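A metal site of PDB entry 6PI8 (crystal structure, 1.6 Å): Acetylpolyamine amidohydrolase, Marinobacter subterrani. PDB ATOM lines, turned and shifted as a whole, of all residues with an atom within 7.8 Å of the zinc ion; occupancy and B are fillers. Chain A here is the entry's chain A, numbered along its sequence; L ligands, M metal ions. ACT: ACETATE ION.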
ATOM      1  N   ARG A  37       4.475 -12.129 -21.597  1.00  0.00           N
ATOM      2  CA  ARG A  37       4.302 -11.486 -22.899  1.00  0.00           C
ATOM      3  C   ARG A  37       3.976 -12.511 -23.964  1.00  0.00           C
ATOM      4  O   ARG A  37       3.006 -12.358 -24.724  1.00  0.00           O
ATOM      5  CB  ARG A  37       5.586 -10.731 -23.293  1.00  0.00           C
ATOM      6  CG  ARG A  37       5.982  -9.584 -22.394  1.00  0.00           C
ATOM      7  CD  ARG A  37       7.331  -8.971 -22.876  1.00  0.00           C
ATOM      8  NE  ARG A  37       7.217  -8.472 -24.238  1.00  0.00           N
ATOM      9  CZ  ARG A  37       7.785  -9.024 -25.304  1.00  0.00           C
ATOM     10  NH1 ARG A  37       8.567 -10.097 -25.199  1.00  0.00           N
ATOM     11  NH2 ARG A  37       7.579  -8.484 -26.501  1.00  0.00           N
ATOM     12  N   PRO A 161      13.290 -11.500 -27.945  1.00  0.00           N
ATOM     13  CA  PRO A 161      13.327 -10.764 -29.215  1.00  0.00           C
ATOM     14  C   PRO A 161      14.726 -10.722 -29.807  1.00  0.00           C
ATOM     15  O   PRO A 161      15.669 -11.271 -29.223  1.00  0.00           O
ATOM     16  CB  PRO A 161      12.861  -9.354 -28.810  1.00  0.00           C
ATOM     17  CG  PRO A 161      13.324  -9.234 -27.359  1.00  0.00           C
ATOM     18  CD  PRO A 161      13.117 -10.622 -26.775  1.00  0.00           C
ATOM     19  N   HIS A 163      15.984  -7.858 -32.546  1.00  0.00           N
ATOM     20  CA  HIS A 163      16.481  -6.851 -33.498  1.00  0.00           C
ATOM     21  C   HIS A 163      17.596  -5.958 -32.958  1.00  0.00           C
ATOM     22  O   HIS A 163      18.203  -5.225 -33.753  1.00  0.00           O
ATOM     23  CB  HIS A 163      15.319  -5.991 -34.049  1.00  0.00           C
ATOM     24  CG  HIS A 163      14.707  -5.046 -33.051  1.00  0.00           C
ATOM     25  ND1 HIS A 163      14.006  -3.928 -33.439  1.00  0.00           N
ATOM     26  CD2 HIS A 163      14.640  -5.081 -31.695  1.00  0.00           C
ATOM     27  CE1 HIS A 163      13.557  -3.302 -32.372  1.00  0.00           C
ATOM     28  NE2 HIS A 163      13.920  -3.978 -31.299  1.00  0.00           N
ATOM     29  N   HIS A 164      17.907  -5.993 -31.664  1.00  0.00           N
ATOM     30  CA  HIS A 164      19.012  -5.182 -31.151  1.00  0.00           C
ATOM     31  C   HIS A 164      20.344  -5.918 -31.168  1.00  0.00           C
ATOM     32  O   HIS A 164      21.380  -5.293 -30.882  1.00  0.00           O
ATOM     33  CB  HIS A 164      18.737  -4.690 -29.713  1.00  0.00           C
ATOM     34  CG  HIS A 164      17.538  -3.794 -29.595  1.00  0.00           C
ATOM     35  ND1 HIS A 164      17.355  -2.669 -30.384  1.00  0.00           N
ATOM     36  CD2 HIS A 164      16.479  -3.834 -28.751  1.00  0.00           C
ATOM     37  CE1 HIS A 164      16.223  -2.073 -30.027  1.00  0.00           C
ATOM     38  NE2 HIS A 164      15.676  -2.765 -29.045  1.00  0.00           N
ATOM     39  N   GLY A 172      19.623  -5.002 -25.178  1.00  0.00           N
ATOM     40  CA  GLY A 172      18.228  -4.615 -25.414  1.00  0.00           C
ATOM     41  C   GLY A 172      17.282  -5.791 -25.403  1.00  0.00           C
ATOM     42  O   GLY A 172      16.329  -5.842 -26.182  1.00  0.00           O
ATOM     43  N   TYR A 173      17.548  -6.769 -24.534  1.00  0.00           N
ATOM     44  CA  TYR A 173      16.768  -7.981 -24.318  1.00  0.00           C
ATOM     45  C   TYR A 173      16.957  -8.999 -25.441  1.00  0.00           C
ATOM     46  O   TYR A 173      16.255 -10.047 -25.437  1.00  0.00           O
ATOM     47  CB  TYR A 173      15.268  -7.688 -24.159  1.00  0.00           C
ATOM     48  CG  TYR A 173      14.907  -6.547 -23.232  1.00  0.00           C
ATOM     49  CD1 TYR A 173      15.680  -6.230 -22.116  1.00  0.00           C
ATOM     50  CD2 TYR A 173      13.759  -5.788 -23.461  1.00  0.00           C
ATOM     51  CE1 TYR A 173      15.341  -5.169 -21.266  1.00  0.00           C
ATOM     52  CE2 TYR A 173      13.399  -4.737 -22.617  1.00  0.00           C
ATOM     53  CZ  TYR A 173      14.183  -4.440 -21.523  1.00  0.00           C
ATOM     54  OH  TYR A 173      13.814  -3.399 -20.697  1.00  0.00           O
ATOM     55  N   ASP A 198      11.229  -2.669 -39.724  1.00  0.00           N
ATOM     56  CA  ASP A 198      11.233  -2.702 -38.262  1.00  0.00           C
ATOM     57  C   ASP A 198      10.237  -1.666 -37.758  1.00  0.00           C
ATOM     58  O   ASP A 198      10.534  -0.464 -37.733  1.00  0.00           O
ATOM     59  CB  ASP A 198      12.662  -2.447 -37.763  1.00  0.00           C
ATOM     60  CG  ASP A 198      12.822  -2.725 -36.277  1.00  0.00           C
ATOM     61  OD1 ASP A 198      11.958  -2.264 -35.505  1.00  0.00           O
ATOM     62  OD2 ASP A 198      13.802  -3.398 -35.873  1.00  0.00           O
ATOM     63  N   VAL A 199       9.040  -2.123 -37.360  1.00  0.00           N
ATOM     64  CA  VAL A 199       7.997  -1.230 -36.861  1.00  0.00           C
ATOM     65  C   VAL A 199       7.926  -1.203 -35.338  1.00  0.00           C
ATOM     66  O   VAL A 199       7.090  -0.492 -34.758  1.00  0.00           O
ATOM     67  CB  VAL A 199       6.618  -1.577 -37.476  1.00  0.00           C
ATOM     68  CG1 VAL A 199       6.666  -1.321 -38.980  1.00  0.00           C
ATOM     69  CG2 VAL A 199       6.239  -3.027 -37.161  1.00  0.00           C
ATOM     70  N   ASP A 200       8.814  -1.937 -34.664  1.00  0.00           N
ATOM     71  CA  ASP A 200       8.998  -1.815 -33.222  1.00  0.00           C
ATOM     72  C   ASP A 200       9.333  -0.372 -32.875  1.00  0.00           C
ATOM     73  O   ASP A 200       9.948   0.352 -33.662  1.00  0.00           O
ATOM     74  CB  ASP A 200      10.115  -2.780 -32.796  1.00  0.00           C
ATOM     75  CG  ASP A 200      10.341  -2.823 -31.312  1.00  0.00           C
ATOM     76  OD1 ASP A 200      11.014  -1.909 -30.782  1.00  0.00           O
ATOM     77  OD2 ASP A 200       9.908  -3.800 -30.671  1.00  0.00           O
ATOM     78  N   PHE A 201       8.932   0.067 -31.671  1.00  0.00           N
ATOM     79  CA  PHE A 201       9.195   1.438 -31.248  1.00  0.00           C
ATOM     80  C   PHE A 201      10.688   1.787 -31.286  1.00  0.00           C
ATOM     81  O   PHE A 201      11.041   2.963 -31.441  1.00  0.00           O
ATOM     82  CB  PHE A 201       8.666   1.663 -29.836  1.00  0.00           C
ATOM     83  CG  PHE A 201       9.157   2.938 -29.207  1.00  0.00           C
ATOM     84  CD1 PHE A 201       8.531   4.142 -29.479  1.00  0.00           C
ATOM     85  CD2 PHE A 201      10.219   2.926 -28.321  1.00  0.00           C
ATOM     86  CE1 PHE A 201       8.982   5.315 -28.901  1.00  0.00           C
ATOM     87  CE2 PHE A 201      10.678   4.089 -27.735  1.00  0.00           C
ATOM     88  CZ  PHE A 201      10.065   5.287 -28.026  1.00  0.00           C
ATOM     89  N   HIS A 202      11.558   0.820 -31.067  1.00  0.00           N
ATOM     90  CA  HIS A 202      12.995   1.072 -30.983  1.00  0.00           C
ATOM     91  C   HIS A 202      13.672   0.790 -32.314  1.00  0.00           C
ATOM     92  O   HIS A 202      13.192   0.005 -33.134  1.00  0.00           O
ATOM     93  CB  HIS A 202      13.652   0.210 -29.896  1.00  0.00           C
ATOM     94  CG  HIS A 202      13.064   0.388 -28.540  1.00  0.00           C
ATOM     95  ND1 HIS A 202      12.011  -0.384 -28.077  1.00  0.00           N
ATOM     96  CD2 HIS A 202      13.370   1.244 -27.535  1.00  0.00           C
ATOM     97  CE1 HIS A 202      11.706  -0.009 -26.842  1.00  0.00           C
ATOM     98  NE2 HIS A 202      12.516   0.983 -26.490  1.00  0.00           N
ATOM     99  N   HIS A 203      14.801   1.445 -32.516  1.00  0.00           N
ATOM    100  CA  HIS A 203      15.607   1.192 -33.695  1.00  0.00           C
ATOM    101  C   HIS A 203      16.108  -0.244 -33.721  1.00  0.00           C
ATOM    102  O   HIS A 203      16.637  -0.733 -32.718  1.00  0.00           O
ATOM    103  CB  HIS A 203      16.797   2.146 -33.731  1.00  0.00           C
ATOM    104  CG  HIS A 203      17.700   1.919 -34.899  1.00  0.00           C
ATOM    105  ND1 HIS A 203      19.069   1.801 -34.785  1.00  0.00           N
ATOM    106  CD2 HIS A 203      17.411   1.767 -36.223  1.00  0.00           C
ATOM    107  CE1 HIS A 203      19.592   1.618 -35.989  1.00  0.00           C
ATOM    108  NE2 HIS A 203      18.614   1.588 -36.874  1.00  0.00           N
ATOM    109  N   PHE A 230      16.857   4.508 -26.057  1.00  0.00           N
ATOM    110  CA  PHE A 230      17.631   3.392 -26.566  1.00  0.00           C
ATOM    111  C   PHE A 230      17.309   3.160 -28.047  1.00  0.00           C
ATOM    112  O   PHE A 230      16.141   3.193 -28.436  1.00  0.00           O
ATOM    113  CB  PHE A 230      17.284   2.136 -25.753  1.00  0.00           C
ATOM    114  CG  PHE A 230      18.120   0.941 -26.095  1.00  0.00           C
ATOM    115  CD1 PHE A 230      19.371   0.768 -25.540  1.00  0.00           C
ATOM    116  CD2 PHE A 230      17.647  -0.007 -26.990  1.00  0.00           C
ATOM    117  CE1 PHE A 230      20.137  -0.333 -25.859  1.00  0.00           C
ATOM    118  CE2 PHE A 230      18.406  -1.104 -27.325  1.00  0.00           C
ATOM    119  CZ  PHE A 230      19.656  -1.265 -26.754  1.00  0.00           C
ATOM    120  N   LEU A 286       8.331  -7.010 -35.697  1.00  0.00           N
ATOM    121  CA  LEU A 286       7.093  -6.445 -35.172  1.00  0.00           C
ATOM    122  C   LEU A 286       7.202  -6.256 -33.661  1.00  0.00           C
ATOM    123  O   LEU A 286       7.257  -7.219 -32.907  1.00  0.00           O
ATOM    124  CB  LEU A 286       5.909  -7.351 -35.503  1.00  0.00           C
ATOM    125  CG  LEU A 286       4.655  -6.864 -34.779  1.00  0.00           C
ATOM    126  CD1 LEU A 286       4.176  -5.546 -35.383  1.00  0.00           C
ATOM    127  CD2 LEU A 286       3.567  -7.897 -34.852  1.00  0.00           C
ATOM    128  N   GLY A 287       7.181  -5.001 -33.232  1.00  0.00           N
ATOM    129  CA  GLY A 287       6.978  -4.672 -31.838  1.00  0.00           C
ATOM    130  C   GLY A 287       5.683  -3.912 -31.686  1.00  0.00           C
ATOM    131  O   GLY A 287       5.286  -3.150 -32.575  1.00  0.00           O
ATOM    132  N   VAL A 288       5.011  -4.119 -30.569  1.00  0.00           N
ATOM    133  CA  VAL A 288       3.832  -3.323 -30.246  1.00  0.00           C
ATOM    134  C   VAL A 288       4.131  -2.406 -29.060  1.00  0.00           C
ATOM    135  O   VAL A 288       3.212  -1.990 -28.357  1.00  0.00           O
ATOM    136  CB  VAL A 288       2.591  -4.197 -30.009  1.00  0.00           C
ATOM    137  CG1 VAL A 288       2.151  -4.836 -31.307  1.00  0.00           C
ATOM    138  CG2 VAL A 288       2.867  -5.278 -28.944  1.00  0.00           C
ATOM    139  N   ASP A 289       5.402  -2.091 -28.833  1.00  0.00           N
ATOM    140  CA  ASP A 289       5.745  -1.070 -27.852  1.00  0.00           C
ATOM    141  C   ASP A 289       5.541   0.340 -28.393  1.00  0.00           C
ATOM    142  O   ASP A 289       5.865   1.306 -27.701  1.00  0.00           O
ATOM    143  CB  ASP A 289       7.178  -1.253 -27.327  1.00  0.00           C
ATOM    144  CG  ASP A 289       8.197  -1.590 -28.413  1.00  0.00           C
ATOM    145  OD1 ASP A 289       7.885  -1.568 -29.621  1.00  0.00           O
ATOM    146  OD2 ASP A 289       9.343  -1.903 -28.024  1.00  0.00           O
ATOM    147  N   THR A 290       4.975   0.459 -29.593  1.00  0.00           N
ATOM    148  CA  THR A 290       4.462   1.729 -30.087  1.00  0.00           C
ATOM    149  C   THR A 290       3.131   2.109 -29.437  1.00  0.00           C
ATOM    150  O   THR A 290       2.608   3.196 -29.712  1.00  0.00           O
ATOM    151  CB  THR A 290       4.283   1.654 -31.603  1.00  0.00           C
ATOM    152  OG1 THR A 290       3.582   0.446 -31.931  1.00  0.00           O
ATOM    153  CG2 THR A 290       5.665   1.649 -32.300  1.00  0.00           C
ATOM    154  N   ASP A 294       2.501   1.721 -23.478  1.00  0.00           N
ATOM    155  CA  ASP A 294       3.727   0.973 -23.265  1.00  0.00           C
ATOM    156  C   ASP A 294       4.560   1.631 -22.169  1.00  0.00           C
ATOM    157  O   ASP A 294       4.758   2.856 -22.195  1.00  0.00           O
ATOM    158  CB  ASP A 294       4.548   0.855 -24.536  1.00  0.00           C
ATOM    159  CG  ASP A 294       5.656  -0.141 -24.379  1.00  0.00           C
ATOM    160  OD1 ASP A 294       6.769   0.265 -23.968  1.00  0.00           O
ATOM    161  OD2 ASP A 294       5.391  -1.346 -24.601  1.00  0.00           O
ATOM    162  N   ILE A 296       7.753   1.746 -21.433  1.00  0.00           N
ATOM    163  CA  ILE A 296       9.098   2.255 -21.657  1.00  0.00           C
ATOM    164  C   ILE A 296       9.205   3.069 -22.944  1.00  0.00           C
ATOM    165  O   ILE A 296      10.313   3.433 -23.352  1.00  0.00           O
ATOM    166  CB  ILE A 296      10.154   1.139 -21.651  1.00  0.00           C
ATOM    167  CG1 ILE A 296       9.916   0.148 -22.801  1.00  0.00           C
ATOM    168  CG2 ILE A 296      10.198   0.421 -20.301  1.00  0.00           C
ATOM    169  CD1 ILE A 296      11.083  -0.813 -23.022  1.00  0.00           C
ATOM    170  N   SER A 297       8.093   3.366 -23.598  1.00  0.00           N
ATOM    171  CA  SER A 297       8.127   3.973 -24.919  1.00  0.00           C
ATOM    172  C   SER A 297       7.176   5.171 -24.956  1.00  0.00           C
ATOM    173  O   SER A 297       6.346   5.348 -24.061  1.00  0.00           O
ATOM    174  CB  SER A 297       7.747   2.942 -25.984  1.00  0.00           C
ATOM    175  OG  SER A 297       8.442   1.719 -25.756  1.00  0.00           O
ATOM    176  N   GLU A 325       9.063  -8.782 -31.635  1.00  0.00           N
ATOM    177  CA  GLU A 325      10.113  -8.048 -30.939  1.00  0.00           C
ATOM    178  C   GLU A 325       9.576  -7.558 -29.594  1.00  0.00           C
ATOM    179  O   GLU A 325       9.190  -8.391 -28.757  1.00  0.00           O
ATOM    180  CB  GLU A 325      10.620  -6.889 -31.806  1.00  0.00           C
ATOM    181  CG  GLU A 325      11.103  -7.328 -33.194  1.00  0.00           C
ATOM    182  CD  GLU A 325      12.387  -8.163 -33.175  1.00  0.00           C
ATOM    183  OE1 GLU A 325      13.142  -8.123 -32.175  1.00  0.00           O
ATOM    184  OE2 GLU A 325      12.650  -8.871 -34.179  1.00  0.00           O
ATOM    185  N   GLY A 326       9.498  -6.247 -29.377  1.00  0.00           N
ATOM    186  CA  GLY A 326       9.079  -5.701 -28.093  1.00  0.00           C
ATOM    187  C   GLY A 326       7.564  -5.511 -27.955  1.00  0.00           C
ATOM    188  O   GLY A 326       6.767  -5.916 -28.802  1.00  0.00           O
ATOM    189  N   GLY A 327       7.189  -4.875 -26.840  1.00  0.00           N
ATOM    190  CA  GLY A 327       5.803  -4.656 -26.412  1.00  0.00           C
ATOM    191  C   GLY A 327       5.641  -5.081 -24.962  1.00  0.00           C
ATOM    192  O   GLY A 327       5.774  -6.269 -24.661  1.00  0.00           O
ATOM    193  N   TYR A 328       5.376  -4.144 -24.035  1.00  0.00           N
ATOM    194  CA  TYR A 328       5.571  -4.413 -22.605  1.00  0.00           C
ATOM    195  C   TYR A 328       4.367  -4.093 -21.734  1.00  0.00           C
ATOM    196  O   TYR A 328       4.428  -4.330 -20.517  1.00  0.00           O
ATOM    197  CB  TYR A 328       6.824  -3.665 -22.108  1.00  0.00           C
ATOM    198  CG  TYR A 328       8.006  -4.091 -22.923  1.00  0.00           C
ATOM    199  CD1 TYR A 328       8.597  -5.325 -22.707  1.00  0.00           C
ATOM    200  CD2 TYR A 328       8.463  -3.308 -23.983  1.00  0.00           C
ATOM    201  CE1 TYR A 328       9.655  -5.758 -23.487  1.00  0.00           C
ATOM    202  CE2 TYR A 328       9.524  -3.740 -24.777  1.00  0.00           C
ATOM    203  CZ  TYR A 328      10.117  -4.960 -24.507  1.00  0.00           C
ATOM    204  OH  TYR A 328      11.154  -5.403 -25.294  1.00  0.00           O
HETATM  205  C   ACT L   1      12.520  -4.199 -27.937  1.00  0.00           C
HETATM  206  O   ACT L   1      11.704  -3.792 -27.094  1.00  0.00           O
HETATM  207  OXT ACT L   1      12.731  -3.488 -28.933  1.00  0.00           O
HETATM  208  CH3 ACT L   1      13.262  -5.496 -27.750  1.00  0.00           C
HETATM  209 ZN    ZN M   1      11.120  -2.079 -28.814  1.00  0.00          ZN
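OD1 of Asp 289 sits at hydrogen-bond distance from N of Phe 201, at 2.8 Å.
The backbone NH of Gly 326 lies within hydrogen-bond range of the side-chain carboxylate of Asp 200.
The side-chain hydroxyl of Ser 297 sits close to the backbone carbonyl oxygen of Asp 289 (3.3 Å).
The side-chain carboxylate (OD1) of Asp 198 is in hydrogen-bond range of the backbone NH (N) of Asp 200, at 3.3 Å.
Of the 25 residues printed, 3 come within 4 Å of the zinc ion.
The nearest printed residue that does not touch the zinc ion is Phe 201 (4.2 Å).
The zinc ion is bound by OD2 of Asp 289 (2.0 Å), OD1 of Asp 200 (2.0 Å), ND1 of His 202 (2.1 Å), OXT of the ligand (2.1 Å) and O of the ligand (2.5 Å).
The zinc ion has five donor atoms within binding distance.
Slightly farther from the zinc ion lies OD2 of Asp 200 (2.8 Å).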
